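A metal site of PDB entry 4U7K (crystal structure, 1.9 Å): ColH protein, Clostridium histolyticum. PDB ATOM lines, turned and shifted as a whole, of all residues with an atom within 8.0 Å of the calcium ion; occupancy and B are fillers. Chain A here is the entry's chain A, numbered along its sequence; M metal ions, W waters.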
ATOM      1  N   ASN A   2      18.709   1.515 -11.241  1.00  0.00           N
ATOM      2  CA  ASN A   2      20.042   2.194 -11.277  1.00  0.00           C
ATOM      3  C   ASN A   2      19.938   3.713 -11.477  1.00  0.00           C
ATOM      4  O   ASN A   2      19.386   4.157 -12.490  1.00  0.00           O
ATOM      5  CB  ASN A   2      20.941   1.577 -12.366  1.00  0.00           C
ATOM      6  CG  ASN A   2      22.347   2.209 -12.388  1.00  0.00           C
ATOM      7  OD1 ASN A   2      22.960   2.371 -11.330  1.00  0.00           O
ATOM      8  ND2 ASN A   2      22.799   2.665 -13.563  1.00  0.00           N
ATOM      9  N   SER A   3      20.603   4.487 -10.627  1.00  0.00           N
ATOM     10  CA  SER A   3      20.817   5.914 -10.889  1.00  0.00           C
ATOM     11  C   SER A   3      21.986   6.120 -11.859  1.00  0.00           C
ATOM     12  O   SER A   3      23.053   5.529 -11.727  1.00  0.00           O
ATOM     13  CB  SER A   3      21.061   6.683  -9.583  1.00  0.00           C
ATOM     14  OG  SER A   3      21.322   8.054  -9.865  1.00  0.00           O
ATOM     15  N   LEU A   4      21.742   6.913 -12.894  1.00  0.00           N
ATOM     16  CA  LEU A   4      22.800   7.257 -13.816  1.00  0.00           C
ATOM     17  C   LEU A   4      23.873   8.049 -13.071  1.00  0.00           C
ATOM     18  O   LEU A   4      23.557   8.841 -12.169  1.00  0.00           O
ATOM     19  CB  LEU A   4      22.265   8.069 -15.008  1.00  0.00           C
ATOM     20  CG  LEU A   4      21.204   7.349 -15.862  1.00  0.00           C
ATOM     21  CD1 LEU A   4      20.710   8.259 -16.969  1.00  0.00           C
ATOM     22  CD2 LEU A   4      21.751   6.066 -16.456  1.00  0.00           C
ATOM     23  N   PRO A   5      25.123   7.961 -13.529  1.00  0.00           N
ATOM     24  CA  PRO A   5      26.167   8.793 -12.921  1.00  0.00           C
ATOM     25  C   PRO A   5      26.024  10.256 -13.350  1.00  0.00           C
ATOM     26  O   PRO A   5      25.477  10.535 -14.420  1.00  0.00           O
ATOM     27  CB  PRO A   5      27.449   8.197 -13.472  1.00  0.00           C
ATOM     28  CG  PRO A   5      27.026   7.613 -14.811  1.00  0.00           C
ATOM     29  CD  PRO A   5      25.668   7.043 -14.550  1.00  0.00           C
ATOM     30  N   TYR A   6      26.587  11.161 -12.536  1.00  0.00           N
ATOM     31  CA  TYR A   6      26.717  12.572 -12.864  1.00  0.00           C
ATOM     32  C   TYR A   6      28.164  12.824 -13.339  1.00  0.00           C
ATOM     33  O   TYR A   6      29.084  12.643 -12.565  1.00  0.00           O
ATOM     34  CB  TYR A   6      26.481  13.425 -11.626  1.00  0.00           C
ATOM     35  CG  TYR A   6      25.057  13.455 -11.143  1.00  0.00           C
ATOM     36  CD1 TYR A   6      24.593  12.485 -10.258  1.00  0.00           C
ATOM     37  CD2 TYR A   6      24.226  14.552 -11.406  1.00  0.00           C
ATOM     38  CE1 TYR A   6      23.359  12.610  -9.623  1.00  0.00           C
ATOM     39  CE2 TYR A   6      22.928  14.628 -10.840  1.00  0.00           C
ATOM     40  CZ  TYR A   6      22.503  13.632  -9.980  1.00  0.00           C
ATOM     41  OH  TYR A   6      21.265  13.704  -9.377  1.00  0.00           O
ATOM     42  N   PHE A  29      30.370  11.850 -10.042  1.00  0.00           N
ATOM     43  CA  PHE A  29      30.090  10.811  -9.054  1.00  0.00           C
ATOM     44  C   PHE A  29      28.911   9.968  -9.494  1.00  0.00           C
ATOM     45  O   PHE A  29      28.157  10.352 -10.385  1.00  0.00           O
ATOM     46  CB  PHE A  29      29.808  11.421  -7.668  1.00  0.00           C
ATOM     47  CG  PHE A  29      28.473  12.134  -7.563  1.00  0.00           C
ATOM     48  CD1 PHE A  29      27.403  11.515  -6.908  1.00  0.00           C
ATOM     49  CD2 PHE A  29      28.278  13.395  -8.121  1.00  0.00           C
ATOM     50  CE1 PHE A  29      26.159  12.126  -6.837  1.00  0.00           C
ATOM     51  CE2 PHE A  29      27.027  14.032  -8.042  1.00  0.00           C
ATOM     52  CZ  PHE A  29      25.972  13.398  -7.400  1.00  0.00           C
ATOM     53  N   ASP A  30      28.743   8.838  -8.822  1.00  0.00           N
ATOM     54  CA  ASP A  30      27.590   7.973  -9.023  1.00  0.00           C
ATOM     55  C   ASP A  30      26.950   7.747  -7.656  1.00  0.00           C
ATOM     56  O   ASP A  30      27.610   7.234  -6.735  1.00  0.00           O
ATOM     57  CB  ASP A  30      28.067   6.632  -9.592  1.00  0.00           C
ATOM     58  CG  ASP A  30      26.898   5.750 -10.045  1.00  0.00           C
ATOM     59  OD1 ASP A  30      25.845   6.294 -10.320  1.00  0.00           O
ATOM     60  OD2 ASP A  30      27.045   4.520 -10.105  1.00  0.00           O
ATOM     61  N   PRO A  31      25.675   8.125  -7.517  1.00  0.00           N
ATOM     62  CA  PRO A  31      25.022   8.052  -6.203  1.00  0.00           C
ATOM     63  C   PRO A  31      25.009   6.633  -5.646  1.00  0.00           C
ATOM     64  O   PRO A  31      24.939   6.457  -4.435  1.00  0.00           O
ATOM     65  CB  PRO A  31      23.571   8.496  -6.489  1.00  0.00           C
ATOM     66  CG  PRO A  31      23.573   9.135  -7.772  1.00  0.00           C
ATOM     67  CD  PRO A  31      24.824   8.738  -8.546  1.00  0.00           C
ATOM     68  N   ASP A  32      24.845   5.643  -6.519  1.00  0.00           N
ATOM     69  CA  ASP A  32      24.598   4.272  -6.043  1.00  0.00           C
ATOM     70  C   ASP A  32      25.573   3.276  -6.672  1.00  0.00           C
ATOM     71  O   ASP A  32      25.249   2.117  -6.871  1.00  0.00           O
ATOM     72  CB  ASP A  32      23.169   3.851  -6.360  1.00  0.00           C
ATOM     73  CG  ASP A  32      22.895   3.802  -7.850  1.00  0.00           C
ATOM     74  OD1 ASP A  32      23.817   4.149  -8.644  1.00  0.00           O
ATOM     75  OD2 ASP A  32      21.791   3.343  -8.240  1.00  0.00           O
ATOM     76  N   GLY A  33      26.792   3.738  -6.911  1.00  0.00           N
ATOM     77  CA  GLY A  33      27.874   2.857  -7.314  1.00  0.00           C
ATOM     78  C   GLY A  33      29.135   3.679  -7.532  1.00  0.00           C
ATOM     79  O   GLY A  33      29.369   4.649  -6.815  1.00  0.00           O
ATOM     80  N   LYS A  34      29.851   3.417  -8.611  1.00  0.00           N
ATOM     81  CA  LYS A  34      31.048   4.191  -8.898  1.00  0.00           C
ATOM     82  C   LYS A  34      31.186   4.398 -10.390  1.00  0.00           C
ATOM     83  O   LYS A  34      30.787   3.534 -11.190  1.00  0.00           O
ATOM     84  CB  LYS A  34      32.275   3.474  -8.339  1.00  0.00           C
ATOM     85  CG  LYS A  34      32.545   2.122  -9.001  1.00  0.00           C
ATOM     86  CD  LYS A  34      33.431   1.223  -8.145  1.00  0.00           C
ATOM     87  CE  LYS A  34      33.709  -0.104  -8.851  1.00  0.00           C
ATOM     88  NZ  LYS A  34      34.280  -1.129  -7.934  1.00  0.00           N
ATOM     89  N   ILE A  35      31.825   5.498 -10.795  1.00  0.00           N
ATOM     90  CA  ILE A  35      32.161   5.671 -12.210  1.00  0.00           C
ATOM     91  C   ILE A  35      33.379   4.847 -12.556  1.00  0.00           C
ATOM     92  O   ILE A  35      34.375   4.878 -11.843  1.00  0.00           O
ATOM     93  CB  ILE A  35      32.400   7.151 -12.559  1.00  0.00           C
ATOM     94  CG1 ILE A  35      31.079   7.923 -12.433  1.00  0.00           C
ATOM     95  CG2 ILE A  35      32.994   7.292 -13.984  1.00  0.00           C
ATOM     96  CD1 ILE A  35      31.228   9.417 -12.492  1.00  0.00           C
ATOM     97  N   THR A  70      30.619   6.431 -17.325  1.00  0.00           N
ATOM     98  CA  THR A  70      29.875   5.171 -17.282  1.00  0.00           C
ATOM     99  C   THR A  70      30.080   4.552 -15.932  1.00  0.00           C
ATOM    100  O   THR A  70      31.205   4.547 -15.411  1.00  0.00           O
ATOM    101  CB  THR A  70      30.376   4.195 -18.353  1.00  0.00           C
ATOM    102  OG1 THR A  70      30.316   4.832 -19.636  1.00  0.00           O
ATOM    103  CG2 THR A  70      29.520   2.912 -18.377  1.00  0.00           C
ATOM    104  N   ASP A  71      28.987   4.084 -15.330  1.00  0.00           N
ATOM    105  CA  ASP A  71      29.057   3.510 -13.994  1.00  0.00           C
ATOM    106  C   ASP A  71      29.270   1.996 -13.987  1.00  0.00           C
ATOM    107  O   ASP A  71      29.387   1.354 -15.055  1.00  0.00           O
ATOM    108  CB  ASP A  71      27.848   3.954 -13.122  1.00  0.00           C
ATOM    109  CG  ASP A  71      26.519   3.346 -13.578  1.00  0.00           C
ATOM    110  OD1 ASP A  71      26.498   2.373 -14.363  1.00  0.00           O
ATOM    111  OD2 ASP A  71      25.463   3.796 -13.070  1.00  0.00           O
ATOM    112  N   ASP A  72      29.249   1.418 -12.780  1.00  0.00           N
ATOM    113  CA  ASP A  72      29.554   0.024 -12.642  1.00  0.00           C
ATOM    114  C   ASP A  72      28.403  -0.858 -13.170  1.00  0.00           C
ATOM    115  O   ASP A  72      28.537  -2.074 -13.239  1.00  0.00           O
ATOM    116  CB  ASP A  72      29.844  -0.274 -11.166  1.00  0.00           C
ATOM    117  CG  ASP A  72      28.700   0.148 -10.271  1.00  0.00           C
ATOM    118  OD1 ASP A  72      28.399   1.368 -10.193  1.00  0.00           O
ATOM    119  OD2 ASP A  72      27.972  -0.748  -9.787  1.00  0.00           O
ATOM    120  N   LYS A  73      27.246  -0.262 -13.479  1.00  0.00           N
ATOM    121  CA  LYS A  73      26.131  -1.010 -14.096  1.00  0.00           C
ATOM    122  C   LYS A  73      26.165  -0.917 -15.613  1.00  0.00           C
ATOM    123  O   LYS A  73      25.329  -1.512 -16.312  1.00  0.00           O
ATOM    124  CB  LYS A  73      24.775  -0.524 -13.575  1.00  0.00           C
ATOM    125  CG  LYS A  73      24.526  -0.856 -12.103  1.00  0.00           C
ATOM    126  CD  LYS A  73      24.711  -2.349 -11.842  1.00  0.00           C
ATOM    127  CE  LYS A  73      24.962  -2.620 -10.365  1.00  0.00           C
ATOM    128  NZ  LYS A  73      23.697  -2.859  -9.623  1.00  0.00           N
ATOM    129  N   GLY A  74      27.132  -0.177 -16.143  1.00  0.00           N
ATOM    130  CA  GLY A  74      27.277  -0.056 -17.583  1.00  0.00           C
ATOM    131  C   GLY A  74      26.411   1.042 -18.168  1.00  0.00           C
ATOM    132  O   GLY A  74      26.266   1.127 -19.380  1.00  0.00           O
ATOM    133  N   GLU A  75      25.857   1.894 -17.319  1.00  0.00           N
ATOM    134  CA  GLU A  75      25.027   3.014 -17.784  1.00  0.00           C
ATOM    135  C   GLU A  75      25.752   4.352 -17.711  1.00  0.00           C
ATOM    136  O   GLU A  75      26.661   4.528 -16.880  1.00  0.00           O
ATOM    137  CB  GLU A  75      23.693   3.049 -17.037  1.00  0.00           C
ATOM    138  CG  GLU A  75      22.927   1.733 -17.185  1.00  0.00           C
ATOM    139  CD  GLU A  75      21.476   1.831 -16.828  1.00  0.00           C
ATOM    140  OE1 GLU A  75      21.155   2.529 -15.838  1.00  0.00           O
ATOM    141  OE2 GLU A  75      20.659   1.199 -17.517  1.00  0.00           O
ATOM    142  N   SER A  76      25.471   5.228 -18.679  1.00  0.00           N
ATOM    143  CA  SER A  76      26.314   6.403 -18.910  1.00  0.00           C
ATOM    144  C   SER A  76      25.511   7.696 -18.978  1.00  0.00           C
ATOM    145  O   SER A  76      24.267   7.685 -19.033  1.00  0.00           O
ATOM    146  CB  SER A  76      27.144   6.248 -20.184  1.00  0.00           C
ATOM    147  OG  SER A  76      27.722   4.958 -20.264  1.00  0.00           O
HETATM  148 CA    CA M   1      24.738   4.119 -10.855  1.00  0.00          CA
HETATM  149  O   HOH W   1      25.753   1.961 -10.375  1.00  0.00           O
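OD1 of Asp 71 sits at hydrogen-bond distance from N of Lys 73, at 2.9 Å. The side-chain carboxylate of Asp 71 lies within hydrogen-bond range of the backbone NH of Glu 75. The side-chain carboxylate (OD1) of Asp 71 lies within hydrogen-bond range of the backbone NH (N) of Gly 74. The backbone NH of Gly 33 lies close to the side-chain carboxylate of Asp 30 (3.3 Å). N of Lys 34 lies close to OD2 of Asp 30 (3.4 Å). The side-chain amide nitrogen of Asn 2 sits at hydrogen-bond distance from the side-chain carboxylate of Glu 75 (2.8 Å).
Within 4 Å of the calcium ion: Asn 2, Ser 3, Asp 30, Asp 32 and Asp 71. The nearest printed residue that does not touch the calcium ion is Gly 33 (4.5 Å).
The calcium ion is bound by the side-chain carboxylate (OD2) of Asp 71, 2.4 Å away. The calcium ion is bound by O of Ser 3 (2.4 Å). OD1 of Asp 32 is bound to the calcium ion, at 2.4 Å. The calcium ion is bound by water W1. The side-chain carboxylate (OD2) of Asp 30 is bound to the calcium ion (2.5 Å). The calcium ion is bound by the side-chain carboxylate (OD1) of Asp 30 (2.5 Å). OD1 of Asn 2 is bound to the calcium ion, 2.5 Å away.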
